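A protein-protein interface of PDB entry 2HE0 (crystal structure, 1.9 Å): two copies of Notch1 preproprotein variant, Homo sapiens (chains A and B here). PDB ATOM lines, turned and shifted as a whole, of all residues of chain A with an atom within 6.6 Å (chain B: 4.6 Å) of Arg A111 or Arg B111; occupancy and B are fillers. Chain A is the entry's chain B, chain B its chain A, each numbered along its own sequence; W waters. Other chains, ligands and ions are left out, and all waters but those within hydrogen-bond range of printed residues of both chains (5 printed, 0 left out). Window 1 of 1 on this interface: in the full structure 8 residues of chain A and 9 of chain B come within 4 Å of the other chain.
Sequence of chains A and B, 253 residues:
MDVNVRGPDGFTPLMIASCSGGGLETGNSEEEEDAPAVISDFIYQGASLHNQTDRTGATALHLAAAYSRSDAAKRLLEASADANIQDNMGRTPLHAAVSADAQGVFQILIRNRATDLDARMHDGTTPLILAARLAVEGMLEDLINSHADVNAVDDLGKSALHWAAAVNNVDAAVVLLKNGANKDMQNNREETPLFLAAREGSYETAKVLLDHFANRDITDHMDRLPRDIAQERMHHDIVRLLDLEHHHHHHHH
The side-chain carboxylate (OE1) of Glu B78 lies within salt-bridge range of the side-chain amino group (NZ) of Lys A74 (3.3 Å).
NE of Arg B113 sits at hydrogen-bond distance from O of Ile A110 (2.7 Å).
O of Ile B110 is in hydrogen-bond range of NE of Arg A113, at 2.7 Å.
The backbone NH (N) of Arg B113 sits at hydrogen-bond distance from the backbone carbonyl oxygen (O) of Arg A111 (2.8 Å).
O of Arg A113 sits at hydrogen-bond distance from NH2 of Arg B113 (3.3 Å).
The backbone carbonyl oxygen of Arg A111 lies close to the backbone carbonyl oxygen of Arg B111 (3.3 Å).
NH2 of Arg A113 is in hydrogen-bond range of O of Asn B112 (2.9 Å).
O of Asn A112 lies within hydrogen-bond range of NH2 of Arg B113, 3.0 Å away.
O of Arg B111 sits at hydrogen-bond distance from N of Arg A113, 2.8 Å away.
O of Thr A115 lies within hydrogen-bond range of NH2 of Arg B113, at 2.7 Å.
The backbone carbonyl oxygen of Leu A109 sits at hydrogen-bond distance from the side-chain hydroxyl of Thr A115 (2.8 Å).
ND2 of Asn A112 lies within hydrogen-bond range of OG1 of Thr A115, 3.2 Å away.
CG of Glu A78 touches NH2 of Arg B111, 3.7 Å away.
Arg A111 touches Glu B78 (NH1 to O, 3.9 Å).
Arg A111 touches Asn B112 (O to CA, 3.4 Å).
O of Arg B111 touches CA of Asn A112, 3.4 Å away.
Leu A117 touches Arg B113.
Of chain B, only Glu B78, Arg B111, Asn B112 and Arg B113 come within 4 Å of Arg A111.
Printed residues of chain A within 4 Å of Arg B111: Glu A78 (3.7 Å), Arg A111 (3.3 Å), Asn A112 (3.4 Å) and Arg A113 (2.8 Å).
Of the printed residues of chain A, Glu B78 touches Lys A74 and Arg A111.
Of the printed residues of chain A, Asn B112 touches Arg A111 (3.4 Å) and Arg A113 (2.9 Å).
Leu A109 touches none of the printed residues of chain B.
The nearest printed residue of chain A that does not touch Asn B112 is Asn A112 (5.3 Å).
Of the 8 printed residues of chain B, 5 touch a printed residue of chain A.
Of the 18 printed residues of chain A, 8 touch a printed residue of chain B.
Printed residues of chain A that touch a printed residue of chain B: Lys A74, Glu A78, Ile A110, Arg A111, Asn A112, Arg A113, Thr A115 and Leu A117.
Hydrophobic or aromatic side chains of chain A within 4 Å of the printed part of chain B: Leu A117.
Among the printed residues, Asp or Glu carboxylates within 4 Å of a Lys or Arg side-chain nitrogen of the other chain: Lys A74 with Glu B78 (3.3 Å).
Glu A78 touches Arg B111, and with the chains exchanged Arg A111 touches Glu B78.
Arg A111 touches its own counterpart, Arg B111.
Arg A111 touches Asn B112, and with the chains exchanged Asn A112 touches Arg B111.
Arg B113 touches its own counterpart, Arg A113.
8 positions are printed for both chains.
Water W5 bridges the backbone carbonyl oxygen (O) of Ser A146 (2.6 Å) and the guanidinium group (NH1) of Arg B113 (2.9 Å).
Water W2 lies within hydrogen-bond range of OD1 of Asn A112 and NE of Arg B111.
Water W1 bridges the backbone carbonyl oxygen of Arg B113 (2.8 Å) and the guanidinium group of Arg A113 (3.1 Å).
Water W3 lies within hydrogen-bond range of the backbone carbonyl oxygen of Arg A113 (2.9 Å), the guanidinium group of Arg B113 (3.0 Å) and the backbone carbonyl oxygen of Thr A115 (3.2 Å).
Water W4 bridges the backbone carbonyl oxygen (O) of Arg A111 (3.0 Å) and the backbone carbonyl oxygen (O) of Arg B111 (3.3 Å).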
ATOM      1  N   LYS A  74     -37.245  -9.132  19.953  1.00  0.00           N
ATOM      2  CA  LYS A  74     -36.147  -8.961  19.000  1.00  0.00           C
ATOM      3  C   LYS A  74     -35.927  -7.464  18.704  1.00  0.00           C
ATOM      4  O   LYS A  74     -34.802  -6.951  18.750  1.00  0.00           O
ATOM      5  CB  LYS A  74     -36.447  -9.717  17.700  1.00  0.00           C
ATOM      6  CG  LYS A  74     -36.032 -11.193  17.753  1.00  0.00           C
ATOM      7  CD  LYS A  74     -35.899 -11.821  16.383  1.00  0.00           C
ATOM      8  CE  LYS A  74     -37.262 -12.144  15.793  1.00  0.00           C
ATOM      9  NZ  LYS A  74     -37.186 -13.266  14.839  1.00  0.00           N
ATOM     10  N   LEU A  77     -34.364  -5.684  21.816  1.00  0.00           N
ATOM     11  CA  LEU A  77     -32.950  -6.045  21.963  1.00  0.00           C
ATOM     12  C   LEU A  77     -32.073  -5.373  20.898  1.00  0.00           C
ATOM     13  O   LEU A  77     -30.979  -4.879  21.201  1.00  0.00           O
ATOM     14  CB  LEU A  77     -32.784  -7.578  21.919  1.00  0.00           C
ATOM     15  CG  LEU A  77     -33.315  -8.214  23.211  1.00  0.00           C
ATOM     16  CD1 LEU A  77     -33.405  -9.766  23.118  1.00  0.00           C
ATOM     17  CD2 LEU A  77     -32.525  -7.770  24.438  1.00  0.00           C
ATOM     18  N   GLU A  78     -32.548  -5.372  19.656  1.00  0.00           N
ATOM     19  CA  GLU A  78     -31.811  -4.736  18.560  1.00  0.00           C
ATOM     20  C   GLU A  78     -31.731  -3.217  18.735  1.00  0.00           C
ATOM     21  O   GLU A  78     -30.803  -2.580  18.200  1.00  0.00           O
ATOM     22  CB  GLU A  78     -32.412  -5.125  17.207  1.00  0.00           C
ATOM     23  CG  GLU A  78     -32.344  -6.630  16.928  1.00  0.00           C
ATOM     24  CD  GLU A  78     -33.255  -7.069  15.794  1.00  0.00           C
ATOM     25  OE1 GLU A  78     -33.767  -6.200  15.054  1.00  0.00           O
ATOM     26  OE2 GLU A  78     -33.467  -8.289  15.630  1.00  0.00           O
ATOM     27  N   ALA A  79     -32.697  -2.655  19.484  1.00  0.00           N
ATOM     28  CA  ALA A  79     -32.704  -1.235  19.937  1.00  0.00           C
ATOM     29  C   ALA A  79     -31.959  -1.012  21.261  1.00  0.00           C
ATOM     30  O   ALA A  79     -32.147   0.014  21.922  1.00  0.00           O
ATOM     31  CB  ALA A  79     -34.142  -0.701  20.050  1.00  0.00           C
ATOM     32  N   SER A  80     -31.144  -1.994  21.646  1.00  0.00           N
ATOM     33  CA  SER A  80     -30.278  -1.952  22.828  1.00  0.00           C
ATOM     34  C   SER A  80     -30.956  -1.818  24.182  1.00  0.00           C
ATOM     35  O   SER A  80     -30.371  -1.243  25.103  1.00  0.00           O
ATOM     36  CB  SER A  80     -29.150  -0.909  22.671  1.00  0.00           C
ATOM     37  OG  SER A  80     -28.003  -1.510  22.088  1.00  0.00           O
ATOM     38  N   GLY A 104     -40.319 -19.051  22.464  1.00  0.00           N
ATOM     39  CA  GLY A 104     -39.738 -18.135  21.468  1.00  0.00           C
ATOM     40  C   GLY A 104     -38.941 -16.976  22.088  1.00  0.00           C
ATOM     41  O   GLY A 104     -37.785 -16.727  21.694  1.00  0.00           O
ATOM     42  N   PHE A 106     -37.877 -16.880  25.316  1.00  0.00           N
ATOM     43  CA  PHE A 106     -36.802 -17.560  26.045  1.00  0.00           C
ATOM     44  C   PHE A 106     -35.586 -17.783  25.151  1.00  0.00           C
ATOM     45  O   PHE A 106     -34.462 -17.499  25.551  1.00  0.00           O
ATOM     46  CB  PHE A 106     -37.306 -18.910  26.620  1.00  0.00           C
ATOM     47  CG  PHE A 106     -36.190 -19.786  27.155  1.00  0.00           C
ATOM     48  CD1 PHE A 106     -35.661 -19.553  28.419  1.00  0.00           C
ATOM     49  CD2 PHE A 106     -35.660 -20.831  26.373  1.00  0.00           C
ATOM     50  CE1 PHE A 106     -34.609 -20.379  28.927  1.00  0.00           C
ATOM     51  CE2 PHE A 106     -34.606 -21.637  26.883  1.00  0.00           C
ATOM     52  CZ  PHE A 106     -34.103 -21.409  28.123  1.00  0.00           C
ATOM     53  N   GLN A 107     -35.806 -18.292  23.933  1.00  0.00           N
ATOM     54  CA  GLN A 107     -34.706 -18.587  23.020  1.00  0.00           C
ATOM     55  C   GLN A 107     -33.996 -17.315  22.539  1.00  0.00           C
ATOM     56  O   GLN A 107     -32.767 -17.249  22.500  1.00  0.00           O
ATOM     57  CB  GLN A 107     -35.198 -19.412  21.814  1.00  0.00           C
ATOM     58  CG  GLN A 107     -35.676 -20.842  22.173  1.00  0.00           C
ATOM     59  CD  GLN A 107     -34.585 -21.739  22.738  1.00  0.00           C
ATOM     60  OE1 GLN A 107     -33.390 -21.553  22.471  1.00  0.00           O
ATOM     61  NE2 GLN A 107     -34.999 -22.745  23.493  1.00  0.00           N
ATOM     62  N   ILE A 108     -34.771 -16.290  22.217  1.00  0.00           N
ATOM     63  CA  ILE A 108     -34.225 -14.975  21.903  1.00  0.00           C
ATOM     64  C   ILE A 108     -33.356 -14.406  23.047  1.00  0.00           C
ATOM     65  O   ILE A 108     -32.257 -13.870  22.835  1.00  0.00           O
ATOM     66  CB  ILE A 108     -35.381 -13.993  21.517  1.00  0.00           C
ATOM     67  CG1 ILE A 108     -36.019 -14.431  20.204  1.00  0.00           C
ATOM     68  CG2 ILE A 108     -34.883 -12.553  21.447  1.00  0.00           C
ATOM     69  CD1 ILE A 108     -37.444 -13.811  20.011  1.00  0.00           C
ATOM     70  N   LEU A 109     -33.855 -14.484  24.262  1.00  0.00           N
ATOM     71  CA  LEU A 109     -33.111 -13.979  25.390  1.00  0.00           C
ATOM     72  C   LEU A 109     -31.804 -14.739  25.684  1.00  0.00           C
ATOM     73  O   LEU A 109     -30.793 -14.124  25.983  1.00  0.00           O
ATOM     74  CB  LEU A 109     -33.978 -13.983  26.620  1.00  0.00           C
ATOM     75  CG  LEU A 109     -35.091 -12.898  26.592  1.00  0.00           C
ATOM     76  CD1 LEU A 109     -35.967 -13.185  27.779  1.00  0.00           C
ATOM     77  CD2 LEU A 109     -34.479 -11.453  26.683  1.00  0.00           C
ATOM     78  N   ILE A 110     -31.834 -16.066  25.631  1.00  0.00           N
ATOM     79  CA  ILE A 110     -30.611 -16.831  25.937  1.00  0.00           C
ATOM     80  C   ILE A 110     -29.585 -16.737  24.805  1.00  0.00           C
ATOM     81  O   ILE A 110     -28.376 -16.873  25.032  1.00  0.00           O
ATOM     82  CB  ILE A 110     -30.862 -18.311  26.352  1.00  0.00           C
ATOM     83  CG1 ILE A 110     -31.273 -19.168  25.146  1.00  0.00           C
ATOM     84  CG2 ILE A 110     -31.782 -18.392  27.644  1.00  0.00           C
ATOM     85  CD1 ILE A 110     -31.334 -20.720  25.425  1.00  0.00           C
ATOM     86  N   ARG A 111     -30.035 -16.443  23.596  1.00  0.00           N
ATOM     87  CA  ARG A 111     -29.092 -16.279  22.478  1.00  0.00           C
ATOM     88  C   ARG A 111     -28.455 -14.878  22.483  1.00  0.00           C
ATOM     89  O   ARG A 111     -27.550 -14.614  21.690  1.00  0.00           O
ATOM     90  CB  ARG A 111     -29.773 -16.476  21.127  1.00  0.00           C
ATOM     91  CG  ARG A 111     -30.298 -17.878  20.796  1.00  0.00           C
ATOM     92  CD  ARG A 111     -30.615 -17.917  19.293  1.00  0.00           C
ATOM     93  NE  ARG A 111     -31.800 -18.726  18.988  1.00  0.00           N
ATOM     94  CZ  ARG A 111     -32.958 -18.259  18.501  1.00  0.00           C
ATOM     95  NH1 ARG A 111     -33.949 -19.119  18.289  1.00  0.00           N
ATOM     96  NH2 ARG A 111     -33.152 -16.956  18.217  1.00  0.00           N
ATOM     97  N   ASN A 112     -28.964 -13.987  23.331  1.00  0.00           N
ATOM     98  CA  ASN A 112     -28.484 -12.594  23.460  1.00  0.00           C
ATOM     99  C   ASN A 112     -27.369 -12.621  24.488  1.00  0.00           C
ATOM    100  O   ASN A 112     -27.594 -12.937  25.661  1.00  0.00           O
ATOM    101  CB  ASN A 112     -29.615 -11.663  23.956  1.00  0.00           C
ATOM    102  CG  ASN A 112     -29.183 -10.216  24.041  1.00  0.00           C
ATOM    103  OD1 ASN A 112     -28.828  -9.593  23.030  1.00  0.00           O
ATOM    104  ND2 ASN A 112     -29.256  -9.663  25.227  1.00  0.00           N
ATOM    105  N   ARG A 113     -26.147 -12.344  24.030  1.00  0.00           N
ATOM    106  CA  ARG A 113     -24.940 -12.484  24.863  1.00  0.00           C
ATOM    107  C   ARG A 113     -25.042 -11.795  26.240  1.00  0.00           C
ATOM    108  O   ARG A 113     -24.621 -12.335  27.261  1.00  0.00           O
ATOM    109  CB  ARG A 113     -23.673 -11.988  24.062  1.00  0.00           C
ATOM    110  CG  ARG A 113     -22.349 -12.114  24.849  1.00  0.00           C
ATOM    111  CD  ARG A 113     -21.186 -11.519  24.067  1.00  0.00           C
ATOM    112  NE  ARG A 113     -21.068 -12.193  22.783  1.00  0.00           N
ATOM    113  CZ  ARG A 113     -20.343 -13.282  22.540  1.00  0.00           C
ATOM    114  NH1 ARG A 113     -19.582 -13.825  23.497  1.00  0.00           N
ATOM    115  NH2 ARG A 113     -20.387 -13.800  21.310  1.00  0.00           N
ATOM    116  N   ALA A 114     -25.605 -10.608  26.265  1.00  0.00           N
ATOM    117  CA  ALA A 114     -25.586  -9.779  27.465  1.00  0.00           C
ATOM    118  C   ALA A 114     -26.603 -10.216  28.553  1.00  0.00           C
ATOM    119  O   ALA A 114     -26.526  -9.794  29.699  1.00  0.00           O
ATOM    120  CB  ALA A 114     -25.789  -8.325  27.072  1.00  0.00           C
ATOM    121  N   THR A 115     -27.534 -11.100  28.205  1.00  0.00           N
ATOM    122  CA  THR A 115     -28.499 -11.587  29.188  1.00  0.00           C
ATOM    123  C   THR A 115     -27.734 -12.359  30.238  1.00  0.00           C
ATOM    124  O   THR A 115     -26.912 -13.241  29.900  1.00  0.00           O
ATOM    125  CB  THR A 115     -29.518 -12.551  28.524  1.00  0.00           C
ATOM    126  OG1 THR A 115     -30.106 -11.876  27.413  1.00  0.00           O
ATOM    127  CG2 THR A 115     -30.611 -12.976  29.490  1.00  0.00           C
ATOM    128  N   LEU A 117     -27.754 -15.116  32.542  1.00  0.00           N
ATOM    129  CA  LEU A 117     -28.443 -16.390  32.689  1.00  0.00           C
ATOM    130  C   LEU A 117     -28.578 -16.775  34.129  1.00  0.00           C
ATOM    131  O   LEU A 117     -29.375 -17.634  34.464  1.00  0.00           O
ATOM    132  CB  LEU A 117     -27.712 -17.527  31.933  1.00  0.00           C
ATOM    133  CG  LEU A 117     -27.421 -17.299  30.435  1.00  0.00           C
ATOM    134  CD1 LEU A 117     -26.664 -18.548  29.873  1.00  0.00           C
ATOM    135  CD2 LEU A 117     -28.698 -17.032  29.629  1.00  0.00           C
ATOM    136  N   SER A 146     -26.191 -23.490  27.662  1.00  0.00           N
ATOM    137  CA  SER A 146     -25.720 -22.094  27.458  1.00  0.00           C
ATOM    138  C   SER A 146     -24.819 -21.656  28.577  1.00  0.00           C
ATOM    139  O   SER A 146     -24.428 -20.493  28.624  1.00  0.00           O
ATOM    140  CB  SER A 146     -26.874 -21.086  27.328  1.00  0.00           C
ATOM    141  OG  SER A 146     -27.638 -21.354  26.192  1.00  0.00           O
ATOM    142  N   GLU B  78     -31.175 -17.163  13.612  1.00  0.00           N
ATOM    143  CA  GLU B  78     -32.417 -17.695  14.210  1.00  0.00           C
ATOM    144  C   GLU B  78     -32.675 -19.172  13.804  1.00  0.00           C
ATOM    145  O   GLU B  78     -33.181 -19.977  14.595  1.00  0.00           O
ATOM    146  CB  GLU B  78     -33.593 -16.797  13.861  1.00  0.00           C
ATOM    147  CG  GLU B  78     -33.555 -15.444  14.564  1.00  0.00           C
ATOM    148  CD  GLU B  78     -34.236 -14.362  13.743  1.00  0.00           C
ATOM    149  OE1 GLU B  78     -35.018 -14.722  12.829  1.00  0.00           O
ATOM    150  OE2 GLU B  78     -33.989 -13.154  13.985  1.00  0.00           O
ATOM    151  N   GLN B 107     -22.571  -6.173  14.587  1.00  0.00           N
ATOM    152  CA  GLN B 107     -23.311  -5.996  15.845  1.00  0.00           C
ATOM    153  C   GLN B 107     -24.167  -7.212  16.146  1.00  0.00           C
ATOM    154  O   GLN B 107     -24.206  -7.691  17.282  1.00  0.00           O
ATOM    155  CB  GLN B 107     -24.152  -4.681  15.848  1.00  0.00           C
ATOM    156  CG  GLN B 107     -23.321  -3.384  15.784  1.00  0.00           C
ATOM    157  CD  GLN B 107     -22.370  -3.176  16.993  1.00  0.00           C
ATOM    158  OE1 GLN B 107     -22.618  -3.643  18.095  1.00  0.00           O
ATOM    159  NE2 GLN B 107     -21.302  -2.427  16.766  1.00  0.00           N
ATOM    160  N   ILE B 108     -24.783  -7.758  15.105  1.00  0.00           N
ATOM    161  CA  ILE B 108     -25.617  -8.965  15.226  1.00  0.00           C
ATOM    162  C   ILE B 108     -24.777 -10.156  15.688  1.00  0.00           C
ATOM    163  O   ILE B 108     -25.178 -10.886  16.585  1.00  0.00           O
ATOM    164  CB  ILE B 108     -26.324  -9.272  13.872  1.00  0.00           C
ATOM    165  CG1 ILE B 108     -27.420  -8.223  13.599  1.00  0.00           C
ATOM    166  CG2 ILE B 108     -26.882 -10.686  13.837  1.00  0.00           C
ATOM    167  CD1 ILE B 108     -27.691  -7.991  12.109  1.00  0.00           C
ATOM    168  N   LEU B 109     -23.584 -10.312  15.102  1.00  0.00           N
ATOM    169  CA  LEU B 109     -22.708 -11.437  15.465  1.00  0.00           C
ATOM    170  C   LEU B 109     -22.214 -11.354  16.893  1.00  0.00           C
ATOM    171  O   LEU B 109     -22.268 -12.362  17.603  1.00  0.00           O
ATOM    172  CB  LEU B 109     -21.564 -11.599  14.444  1.00  0.00           C
ATOM    173  CG  LEU B 109     -21.992 -12.179  13.091  1.00  0.00           C
ATOM    174  CD1 LEU B 109     -20.896 -11.855  12.112  1.00  0.00           C
ATOM    175  CD2 LEU B 109     -22.246 -13.729  13.226  1.00  0.00           C
ATOM    176  N   ILE B 110     -21.774 -10.165  17.336  1.00  0.00           N
ATOM    177  CA  ILE B 110     -21.315  -9.990  18.735  1.00  0.00           C
ATOM    178  C   ILE B 110     -22.421 -10.091  19.777  1.00  0.00           C
ATOM    179  O   ILE B 110     -22.174 -10.533  20.916  1.00  0.00           O
ATOM    180  CB  ILE B 110     -20.366  -8.775  18.951  1.00  0.00           C
ATOM    181  CG1 ILE B 110     -21.093  -7.419  18.807  1.00  0.00           C
ATOM    182  CG2 ILE B 110     -19.197  -8.835  17.949  1.00  0.00           C
ATOM    183  CD1 ILE B 110     -20.257  -6.250  19.449  1.00  0.00           C
ATOM    184  N   ARG B 111     -23.646  -9.743  19.378  1.00  0.00           N
ATOM    185  CA  ARG B 111     -24.800  -9.923  20.257  1.00  0.00           C
ATOM    186  C   ARG B 111     -25.211 -11.393  20.386  1.00  0.00           C
ATOM    187  O   ARG B 111     -25.938 -11.752  21.303  1.00  0.00           O
ATOM    188  CB  ARG B 111     -26.015  -9.096  19.736  1.00  0.00           C
ATOM    189  CG  ARG B 111     -26.051  -7.628  20.205  1.00  0.00           C
ATOM    190  CD  ARG B 111     -27.524  -7.011  20.084  1.00  0.00           C
ATOM    191  NE  ARG B 111     -28.096  -7.182  18.734  1.00  0.00           N
ATOM    192  CZ  ARG B 111     -28.066  -6.288  17.733  1.00  0.00           C
ATOM    193  NH1 ARG B 111     -27.491  -5.093  17.882  1.00  0.00           N
ATOM    194  NH2 ARG B 111     -28.613  -6.595  16.557  1.00  0.00           N
ATOM    195  N   ASN B 112     -24.757 -12.236  19.469  1.00  0.00           N
ATOM    196  CA  ASN B 112     -25.169 -13.657  19.445  1.00  0.00           C
ATOM    197  C   ASN B 112     -24.253 -14.382  20.397  1.00  0.00           C
ATOM    198  O   ASN B 112     -23.045 -14.378  20.185  1.00  0.00           O
ATOM    199  CB  ASN B 112     -25.055 -14.225  18.016  1.00  0.00           C
ATOM    200  CG  ASN B 112     -25.362 -15.704  17.967  1.00  0.00           C
ATOM    201  OD1 ASN B 112     -26.464 -16.100  18.302  1.00  0.00           O
ATOM    202  ND2 ASN B 112     -24.380 -16.526  17.584  1.00  0.00           N
ATOM    203  N   ARG B 113     -24.791 -14.962  21.466  1.00  0.00           N
ATOM    204  CA  ARG B 113     -23.968 -15.580  22.534  1.00  0.00           C
ATOM    205  C   ARG B 113     -23.010 -16.686  22.035  1.00  0.00           C
ATOM    206  O   ARG B 113     -21.866 -16.802  22.526  1.00  0.00           O
ATOM    207  CB  ARG B 113     -24.863 -16.131  23.640  1.00  0.00           C
ATOM    208  CG  ARG B 113     -24.126 -16.782  24.813  1.00  0.00           C
ATOM    209  CD  ARG B 113     -25.125 -17.476  25.784  1.00  0.00           C
ATOM    210  NE  ARG B 113     -26.034 -16.468  26.321  1.00  0.00           N
ATOM    211  CZ  ARG B 113     -25.828 -15.776  27.440  1.00  0.00           C
ATOM    212  NH1 ARG B 113     -24.740 -15.979  28.216  1.00  0.00           N
ATOM    213  NH2 ARG B 113     -26.703 -14.863  27.788  1.00  0.00           N
HETATM  214  O   HOH W   1     -19.113 -16.830  23.021  1.00  0.00           O
HETATM  215  O   HOH W   2     -29.692  -9.526  20.501  1.00  0.00           O
HETATM  216  O   HOH W   3     -23.756 -13.543  29.695  1.00  0.00           O
HETATM  217  O   HOH W   4     -28.653 -12.582  19.702  1.00  0.00           O
HETATM  218  O   HOH W   5     -23.061 -18.291  28.542  1.00  0.00           O
